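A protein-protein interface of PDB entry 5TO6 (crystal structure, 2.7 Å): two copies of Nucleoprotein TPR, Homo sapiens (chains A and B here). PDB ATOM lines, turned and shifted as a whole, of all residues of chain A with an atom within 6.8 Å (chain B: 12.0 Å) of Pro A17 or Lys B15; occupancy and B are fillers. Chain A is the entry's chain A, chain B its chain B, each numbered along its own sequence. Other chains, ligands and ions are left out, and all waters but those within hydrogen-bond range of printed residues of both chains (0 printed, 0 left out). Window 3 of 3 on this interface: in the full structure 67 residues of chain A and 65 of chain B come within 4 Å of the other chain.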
ATOM      1  N   LEU A  13     -32.270  15.593   5.330  1.00  0.00           N
ATOM      2  CA  LEU A  13     -31.661  14.574   4.489  1.00  0.00           C
ATOM      3  C   LEU A  13     -31.552  15.055   3.047  1.00  0.00           C
ATOM      4  O   LEU A  13     -30.507  14.915   2.413  1.00  0.00           O
ATOM      5  CB  LEU A  13     -32.477  13.278   4.575  1.00  0.00           C
ATOM      6  CG  LEU A  13     -31.936  11.954   4.034  1.00  0.00           C
ATOM      7  CD1 LEU A  13     -32.552  10.802   4.812  1.00  0.00           C
ATOM      8  CD2 LEU A  13     -32.223  11.797   2.551  1.00  0.00           C
ATOM      9  N   ASN A  14     -32.641  15.619   2.534  1.00  0.00           N
ATOM     10  CA  ASN A  14     -32.692  16.074   1.150  1.00  0.00           C
ATOM     11  C   ASN A  14     -31.731  17.223   0.852  1.00  0.00           C
ATOM     12  O   ASN A  14     -31.284  17.384  -0.282  1.00  0.00           O
ATOM     13  CB  ASN A  14     -34.120  16.478   0.785  1.00  0.00           C
ATOM     14  CG  ASN A  14     -34.972  15.291   0.385  1.00  0.00           C
ATOM     15  OD1 ASN A  14     -34.680  14.605  -0.594  1.00  0.00           O
ATOM     16  ND2 ASN A  14     -36.027  15.039   1.149  1.00  0.00           N
ATOM     17  N   LYS A  15     -31.404  18.013   1.870  1.00  0.00           N
ATOM     18  CA  LYS A  15     -30.514  19.158   1.690  1.00  0.00           C
ATOM     19  C   LYS A  15     -29.045  18.749   1.751  1.00  0.00           C
ATOM     20  O   LYS A  15     -28.151  19.583   1.620  1.00  0.00           O
ATOM     21  CB  LYS A  15     -30.789  20.234   2.744  1.00  0.00           C
ATOM     22  CG  LYS A  15     -32.183  20.833   2.692  1.00  0.00           C
ATOM     23  CD  LYS A  15     -32.326  21.950   3.717  1.00  0.00           C
ATOM     24  CE  LYS A  15     -33.753  22.463   3.792  1.00  0.00           C
ATOM     25  NZ  LYS A  15     -34.160  23.165   2.543  1.00  0.00           N
ATOM     26  N   LEU A  16     -28.804  17.457   1.942  1.00  0.00           N
ATOM     27  CA  LEU A  16     -27.451  16.925   1.993  1.00  0.00           C
ATOM     28  C   LEU A  16     -26.974  16.607   0.584  1.00  0.00           C
ATOM     29  O   LEU A  16     -27.761  16.143  -0.241  1.00  0.00           O
ATOM     30  CB  LEU A  16     -27.398  15.664   2.857  1.00  0.00           C
ATOM     31  CG  LEU A  16     -27.474  15.788   4.380  1.00  0.00           C
ATOM     32  CD1 LEU A  16     -27.503  14.407   5.014  1.00  0.00           C
ATOM     33  CD2 LEU A  16     -26.312  16.600   4.922  1.00  0.00           C
ATOM     34  N   PRO A  17     -25.694  16.881   0.294  1.00  0.00           N
ATOM     35  CA  PRO A  17     -25.131  16.439  -0.986  1.00  0.00           C
ATOM     36  C   PRO A  17     -25.320  14.933  -1.133  1.00  0.00           C
ATOM     37  O   PRO A  17     -25.250  14.223  -0.132  1.00  0.00           O
ATOM     38  CB  PRO A  17     -23.654  16.821  -0.872  1.00  0.00           C
ATOM     39  CG  PRO A  17     -23.651  17.978   0.087  1.00  0.00           C
ATOM     40  CD  PRO A  17     -24.732  17.669   1.084  1.00  0.00           C
ATOM     41  N   LYS A  18     -25.557  14.457  -2.351  1.00  0.00           N
ATOM     42  CA  LYS A  18     -25.894  13.053  -2.566  1.00  0.00           C
ATOM     43  C   LYS A  18     -24.762  12.113  -2.160  1.00  0.00           C
ATOM     44  O   LYS A  18     -25.007  11.011  -1.669  1.00  0.00           O
ATOM     45  CB  LYS A  18     -26.274  12.816  -4.028  1.00  0.00           C
ATOM     46  CG  LYS A  18     -27.098  11.558  -4.238  1.00  0.00           C
ATOM     47  CD  LYS A  18     -28.360  11.592  -3.390  1.00  0.00           C
ATOM     48  CE  LYS A  18     -29.084  10.255  -3.408  1.00  0.00           C
ATOM     49  NZ  LYS A  18     -30.338  10.297  -2.608  1.00  0.00           N
ATOM     50  N   SER A  19     -23.528  12.555  -2.376  1.00  0.00           N
ATOM     51  CA  SER A  19     -22.357  11.784  -1.981  1.00  0.00           C
ATOM     52  C   SER A  19     -22.348  11.588  -0.470  1.00  0.00           C
ATOM     53  O   SER A  19     -22.006  10.515   0.028  1.00  0.00           O
ATOM     54  CB  SER A  19     -21.073  12.475  -2.441  1.00  0.00           C
ATOM     55  OG  SER A  19     -20.886  13.704  -1.763  1.00  0.00           O
ATOM     56  N   VAL A  20     -22.734  12.634   0.253  1.00  0.00           N
ATOM     57  CA  VAL A  20     -22.795  12.584   1.711  1.00  0.00           C
ATOM     58  C   VAL A  20     -23.874  11.599   2.155  1.00  0.00           C
ATOM     59  O   VAL A  20     -23.638  10.765   3.027  1.00  0.00           O
ATOM     60  CB  VAL A  20     -23.075  13.971   2.320  1.00  0.00           C
ATOM     61  CG1 VAL A  20     -23.320  13.856   3.815  1.00  0.00           C
ATOM     62  CG2 VAL A  20     -21.918  14.915   2.042  1.00  0.00           C
ATOM     63  N   GLN A  21     -25.053  11.709   1.547  1.00  0.00           N
ATOM     64  CA  GLN A  21     -26.176  10.823   1.848  1.00  0.00           C
ATOM     65  C   GLN A  21     -25.794   9.357   1.678  1.00  0.00           C
ATOM     66  O   GLN A  21     -26.085   8.523   2.534  1.00  0.00           O
ATOM     67  CB  GLN A  21     -27.377  11.138   0.946  1.00  0.00           C
ATOM     68  CG  GLN A  21     -27.973  12.524   1.106  1.00  0.00           C
ATOM     69  CD  GLN A  21     -29.151  12.758   0.172  1.00  0.00           C
ATOM     70  OE1 GLN A  21     -29.768  11.811  -0.319  1.00  0.00           O
ATOM     71  NE2 GLN A  21     -29.466  14.024  -0.078  1.00  0.00           N
ATOM     72  N   ASN A  22     -25.142   9.056   0.559  1.00  0.00           N
ATOM     73  CA  ASN A  22     -24.770   7.687   0.221  1.00  0.00           C
ATOM     74  C   ASN A  22     -23.651   7.141   1.105  1.00  0.00           C
ATOM     75  O   ASN A  22     -23.657   5.961   1.454  1.00  0.00           O
ATOM     76  CB  ASN A  22     -24.372   7.598  -1.255  1.00  0.00           C
ATOM     77  CG  ASN A  22     -25.567   7.715  -2.183  1.00  0.00           C
ATOM     78  OD1 ASN A  22     -26.702   7.452  -1.782  1.00  0.00           O
ATOM     79  ND2 ASN A  22     -25.321   8.112  -3.426  1.00  0.00           N
ATOM     80  N   LEU B   4     -17.965  10.459  12.906  1.00  0.00           N
ATOM     81  CA  LEU B   4     -18.393  11.143  11.690  1.00  0.00           C
ATOM     82  C   LEU B   4     -17.203  11.659  10.884  1.00  0.00           C
ATOM     83  O   LEU B   4     -17.276  11.783   9.661  1.00  0.00           O
ATOM     84  CB  LEU B   4     -19.333  12.301  12.034  1.00  0.00           C
ATOM     85  CG  LEU B   4     -20.038  13.017  10.878  1.00  0.00           C
ATOM     86  CD1 LEU B   4     -20.767  12.028   9.982  1.00  0.00           C
ATOM     87  CD2 LEU B   4     -21.000  14.076  11.401  1.00  0.00           C
ATOM     88  N   VAL B   7     -16.130   8.926   8.571  1.00  0.00           N
ATOM     89  CA  VAL B   7     -17.099   8.610   7.527  1.00  0.00           C
ATOM     90  C   VAL B   7     -17.077   9.638   6.404  1.00  0.00           C
ATOM     91  O   VAL B   7     -17.109   9.282   5.225  1.00  0.00           O
ATOM     92  CB  VAL B   7     -18.528   8.526   8.098  1.00  0.00           C
ATOM     93  CG1 VAL B   7     -19.518   8.128   7.011  1.00  0.00           C
ATOM     94  CG2 VAL B   7     -18.575   7.544   9.252  1.00  0.00           C
ATOM     95  N   LEU B   8     -17.008  10.912   6.770  1.00  0.00           N
ATOM     96  CA  LEU B   8     -17.075  11.982   5.783  1.00  0.00           C
ATOM     97  C   LEU B   8     -15.741  12.704   5.662  1.00  0.00           C
ATOM     98  O   LEU B   8     -14.969  12.779   6.619  1.00  0.00           O
ATOM     99  CB  LEU B   8     -18.176  12.987   6.142  1.00  0.00           C
ATOM    100  CG  LEU B   8     -19.617  12.478   6.200  1.00  0.00           C
ATOM    101  CD1 LEU B   8     -20.558  13.577   6.664  1.00  0.00           C
ATOM    102  CD2 LEU B   8     -20.046  11.944   4.849  1.00  0.00           C
ATOM    103  N   GLU B   9     -15.479  13.231   4.471  1.00  0.00           N
ATOM    104  CA  GLU B   9     -14.281  14.016   4.226  1.00  0.00           C
ATOM    105  C   GLU B   9     -14.416  15.366   4.917  1.00  0.00           C
ATOM    106  O   GLU B   9     -15.529  15.854   5.118  1.00  0.00           O
ATOM    107  CB  GLU B   9     -14.048  14.192   2.725  1.00  0.00           C
ATOM    108  CG  GLU B   9     -13.809  12.883   1.980  1.00  0.00           C
ATOM    109  CD  GLU B   9     -13.698  13.076   0.481  1.00  0.00           C
ATOM    110  OE1 GLU B   9     -13.844  14.227   0.019  1.00  0.00           O
ATOM    111  OE2 GLU B   9     -13.470  12.080  -0.237  1.00  0.00           O
ATOM    112  N   ARG B  10     -13.285  15.952   5.293  1.00  0.00           N
ATOM    113  CA  ARG B  10     -13.263  17.206   6.040  1.00  0.00           C
ATOM    114  C   ARG B  10     -14.002  18.325   5.309  1.00  0.00           C
ATOM    115  O   ARG B  10     -14.629  19.180   5.936  1.00  0.00           O
ATOM    116  CB  ARG B  10     -11.817  17.628   6.315  1.00  0.00           C
ATOM    117  CG  ARG B  10     -11.672  18.823   7.245  1.00  0.00           C
ATOM    118  CD  ARG B  10     -12.366  18.595   8.575  1.00  0.00           C
ATOM    119  NE  ARG B  10     -12.293  19.785   9.418  1.00  0.00           N
ATOM    120  CZ  ARG B  10     -13.153  20.795   9.356  1.00  0.00           C
ATOM    121  NH1 ARG B  10     -14.157  20.763   8.491  1.00  0.00           N
ATOM    122  NH2 ARG B  10     -13.011  21.841  10.161  1.00  0.00           N
ATOM    123  N   THR B  11     -13.930  18.310   3.983  1.00  0.00           N
ATOM    124  CA  THR B  11     -14.558  19.345   3.172  1.00  0.00           C
ATOM    125  C   THR B  11     -16.082  19.240   3.142  1.00  0.00           C
ATOM    126  O   THR B  11     -16.781  20.213   3.429  1.00  0.00           O
ATOM    127  CB  THR B  11     -14.035  19.304   1.724  1.00  0.00           C
ATOM    128  OG1 THR B  11     -12.610  19.455   1.727  1.00  0.00           O
ATOM    129  CG2 THR B  11     -14.662  20.418   0.901  1.00  0.00           C
ATOM    130  N   GLU B  12     -16.596  18.061   2.808  1.00  0.00           N
ATOM    131  CA  GLU B  12     -18.039  17.864   2.683  1.00  0.00           C
ATOM    132  C   GLU B  12     -18.737  17.903   4.040  1.00  0.00           C
ATOM    133  O   GLU B  12     -19.949  18.103   4.118  1.00  0.00           O
ATOM    134  CB  GLU B  12     -18.343  16.544   1.973  1.00  0.00           C
ATOM    135  CG  GLU B  12     -17.709  15.327   2.613  1.00  0.00           C
ATOM    136  CD  GLU B  12     -17.945  14.070   1.802  1.00  0.00           C
ATOM    137  OE1 GLU B  12     -18.659  14.150   0.779  1.00  0.00           O
ATOM    138  OE2 GLU B  12     -17.418  13.004   2.184  1.00  0.00           O
ATOM    139  N   LEU B  13     -17.966  17.696   5.100  1.00  0.00           N
ATOM    140  CA  LEU B  13     -18.483  17.761   6.461  1.00  0.00           C
ATOM    141  C   LEU B  13     -18.955  19.176   6.819  1.00  0.00           C
ATOM    142  O   LEU B  13     -19.897  19.342   7.595  1.00  0.00           O
ATOM    143  CB  LEU B  13     -17.417  17.283   7.453  1.00  0.00           C
ATOM    144  CG  LEU B  13     -17.833  17.159   8.920  1.00  0.00           C
ATOM    145  CD1 LEU B  13     -19.066  16.280   9.045  1.00  0.00           C
ATOM    146  CD2 LEU B  13     -16.691  16.601   9.757  1.00  0.00           C
ATOM    147  N   ASN B  14     -18.298  20.188   6.252  1.00  0.00           N
ATOM    148  CA  ASN B  14     -18.633  21.588   6.527  1.00  0.00           C
ATOM    149  C   ASN B  14     -20.038  22.015   6.098  1.00  0.00           C
ATOM    150  O   ASN B  14     -20.637  22.883   6.732  1.00  0.00           O
ATOM    151  CB  ASN B  14     -17.612  22.519   5.864  1.00  0.00           C
ATOM    152  CG  ASN B  14     -16.320  22.630   6.652  1.00  0.00           C
ATOM    153  OD1 ASN B  14     -15.501  21.713   6.663  1.00  0.00           O
ATOM    154  ND2 ASN B  14     -16.129  23.767   7.313  1.00  0.00           N
ATOM    155  N   LYS B  15     -20.567  21.419   5.032  1.00  0.00           N
ATOM    156  CA  LYS B  15     -21.878  21.823   4.525  1.00  0.00           C
ATOM    157  C   LYS B  15     -23.007  21.418   5.463  1.00  0.00           C
ATOM    158  O   LYS B  15     -24.146  21.852   5.298  1.00  0.00           O
ATOM    159  CB  LYS B  15     -22.148  21.231   3.137  1.00  0.00           C
ATOM    160  CG  LYS B  15     -21.223  21.709   2.034  1.00  0.00           C
ATOM    161  CD  LYS B  15     -21.681  21.157   0.689  1.00  0.00           C
ATOM    162  CE  LYS B  15     -20.640  21.352  -0.400  1.00  0.00           C
ATOM    163  NZ  LYS B  15     -21.141  20.864  -1.716  1.00  0.00           N
ATOM    164  N   LEU B  16     -22.688  20.588   6.448  1.00  0.00           N
ATOM    165  CA  LEU B  16     -23.696  20.092   7.372  1.00  0.00           C
ATOM    166  C   LEU B  16     -23.981  21.081   8.501  1.00  0.00           C
ATOM    167  O   LEU B  16     -23.057  21.640   9.093  1.00  0.00           O
ATOM    168  CB  LEU B  16     -23.254  18.749   7.958  1.00  0.00           C
ATOM    169  CG  LEU B  16     -23.582  17.497   7.138  1.00  0.00           C
ATOM    170  CD1 LEU B  16     -22.715  17.406   5.888  1.00  0.00           C
ATOM    171  CD2 LEU B  16     -23.428  16.246   7.988  1.00  0.00           C
ATOM    172  N   PRO B  17     -25.271  21.297   8.796  1.00  0.00           N
ATOM    173  CA  PRO B  17     -25.755  22.084   9.936  1.00  0.00           C
ATOM    174  C   PRO B  17     -25.328  21.486  11.277  1.00  0.00           C
ATOM    175  O   PRO B  17     -25.148  20.273  11.375  1.00  0.00           O
ATOM    176  CB  PRO B  17     -27.280  22.043   9.776  1.00  0.00           C
ATOM    177  CG  PRO B  17     -27.505  21.745   8.336  1.00  0.00           C
ATOM    178  CD  PRO B  17     -26.377  20.851   7.930  1.00  0.00           C
ATOM    179  N   LYS B  18     -25.166  22.335  12.288  1.00  0.00           N
ATOM    180  CA  LYS B  18     -24.756  21.900  13.620  1.00  0.00           C
ATOM    181  C   LYS B  18     -25.706  20.864  14.211  1.00  0.00           C
ATOM    182  O   LYS B  18     -25.270  19.900  14.843  1.00  0.00           O
ATOM    183  CB  LYS B  18     -24.670  23.112  14.555  1.00  0.00           C
ATOM    184  CG  LYS B  18     -24.483  22.783  16.032  1.00  0.00           C
ATOM    185  CD  LYS B  18     -23.149  22.138  16.351  1.00  0.00           C
ATOM    186  CE  LYS B  18     -22.999  21.985  17.860  1.00  0.00           C
ATOM    187  NZ  LYS B  18     -21.617  21.627  18.282  1.00  0.00           N
ATOM    188  N   SER B  19     -27.003  21.065  14.003  1.00  0.00           N
ATOM    189  CA  SER B  19     -28.012  20.126  14.480  1.00  0.00           C
ATOM    190  C   SER B  19     -27.878  18.753  13.820  1.00  0.00           C
ATOM    191  O   SER B  19     -28.009  17.719  14.479  1.00  0.00           O
ATOM    192  CB  SER B  19     -29.416  20.682  14.235  1.00  0.00           C
ATOM    193  OG  SER B  19     -29.725  20.691  12.853  1.00  0.00           O
ATOM    194  N   VAL B  20     -27.612  18.756  12.517  1.00  0.00           N
ATOM    195  CA  VAL B  20     -27.481  17.523  11.751  1.00  0.00           C
ATOM    196  C   VAL B  20     -26.240  16.739  12.173  1.00  0.00           C
ATOM    197  O   VAL B  20     -26.296  15.519  12.336  1.00  0.00           O
ATOM    198  CB  VAL B  20     -27.426  17.809  10.236  1.00  0.00           C
ATOM    199  CG1 VAL B  20     -27.121  16.541   9.459  1.00  0.00           C
ATOM    200  CG2 VAL B  20     -28.738  18.414   9.767  1.00  0.00           C
ATOM    201  N   GLN B  21     -25.125  17.445  12.346  1.00  0.00           N
ATOM    202  CA  GLN B  21     -23.891  16.828  12.823  1.00  0.00           C
ATOM    203  C   GLN B  21     -24.106  16.133  14.168  1.00  0.00           C
ATOM    204  O   GLN B  21     -23.664  14.999  14.366  1.00  0.00           O
ATOM    205  CB  GLN B  21     -22.769  17.865  12.943  1.00  0.00           C
ATOM    206  CG  GLN B  21     -22.286  18.428  11.614  1.00  0.00           C
ATOM    207  CD  GLN B  21     -21.132  19.406  11.774  1.00  0.00           C
ATOM    208  OE1 GLN B  21     -20.406  19.367  12.767  1.00  0.00           O
ATOM    209  NE2 GLN B  21     -20.955  20.284  10.791  1.00  0.00           N
ATOM    210  N   ASN B  22     -24.786  16.817  15.085  1.00  0.00           N
ATOM    211  CA  ASN B  22     -25.053  16.264  16.408  1.00  0.00           C
ATOM    212  C   ASN B  22     -25.928  15.016  16.353  1.00  0.00           C
ATOM    213  O   ASN B  22     -25.667  14.043  17.059  1.00  0.00           O
ATOM    214  CB  ASN B  22     -25.710  17.313  17.310  1.00  0.00           C
ATOM    215  CG  ASN B  22     -24.790  18.477  17.620  1.00  0.00           C
ATOM    216  OD1 ASN B  22     -25.243  19.603  17.829  1.00  0.00           O
ATOM    217  ND2 ASN B  22     -23.488  18.212  17.650  1.00  0.00           N
ATOM    218  N   LEU B  24     -26.171  12.992  13.798  1.00  0.00           N
ATOM    219  CA  LEU B  24     -25.367  11.971  13.143  1.00  0.00           C
ATOM    220  C   LEU B  24     -24.266  11.424  14.043  1.00  0.00           C
ATOM    221  O   LEU B  24     -24.121  10.207  14.183  1.00  0.00           O
ATOM    222  CB  LEU B  24     -24.762  12.535  11.860  1.00  0.00           C
ATOM    223  CG  LEU B  24     -25.773  12.793  10.744  1.00  0.00           C
ATOM    224  CD1 LEU B  24     -25.081  13.405   9.543  1.00  0.00           C
ATOM    225  CD2 LEU B  24     -26.495  11.509  10.364  1.00  0.00           C
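OG of Ser A19 is in hydrogen-bond range of OE1 of Glu B12, 3.4 Å away.
The backbone carbonyl oxygen (O) of Leu A16 is in hydrogen-bond range of the side-chain amide nitrogen (NE2) of Gln A21, 2.7 Å away.
The side-chain carboxylate of Glu B12 sits at hydrogen-bond distance from the backbone NH of Glu B9 (3.0 Å).
O of Leu B16 is in hydrogen-bond range of NE2 of Gln B21 (3.0 Å).
Among the printed residues, pairs that only touch across the chains: Val A20 with Glu B12 (3.6 Å), Leu A16 with Leu B16 (3.6 Å), Pro A17 with Lys B15 (3.8 Å) and Val A20 with Leu B8 (3.9 Å).
Of chain A, only Pro A17 comes within 4 Å of Lys B15.
Of chain B, only Leu B16 (3.6 Å) comes within 4 Å of Leu A16.
Ser A19 touches one residue of chain B.
Val A20 touches two residues of chain B.
No residue of chain B comes within 4 Å of Gln A21.
Printed residues of chain A within 4 Å of Glu B12: Ser A19 and Val A20.
Printed residues of chain A within 4 Å of Leu B16: Leu A16.
Of the printed residues of chain A, Leu B8 touches Val A20 (3.9 Å).
Leu B24 touches none of the printed residues of chain A.
Glu B9 touches none of the printed residues of chain A.
Of the 10 printed residues of chain A, 4 touch a printed residue of chain B.
Printed residues of chain A that touch a printed residue of chain B: Leu A16, Pro A17, Ser A19 and Val A20.
Hydrophobic or aromatic side chains of chain A within 4 Å of the printed part of chain B: Leu A16, Pro A17 and Val A20.
Of the 18 printed residues of chain B, 4 touch a printed residue of chain A.
Hydrophobic or aromatic side chains of chain B within 4 Å of the printed part of chain A: Leu B8 and Leu B16.
Among the printed residues, no Asp or Glu carboxylate lies within 4 Å of a Lys or Arg side-chain nitrogen of the other chain.
Leu A16 touches its own counterpart, Leu B16.
Pro A17 touches Lys B15, but with the chains exchanged Lys A15 does not touch Pro B17 (6.7 Å).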
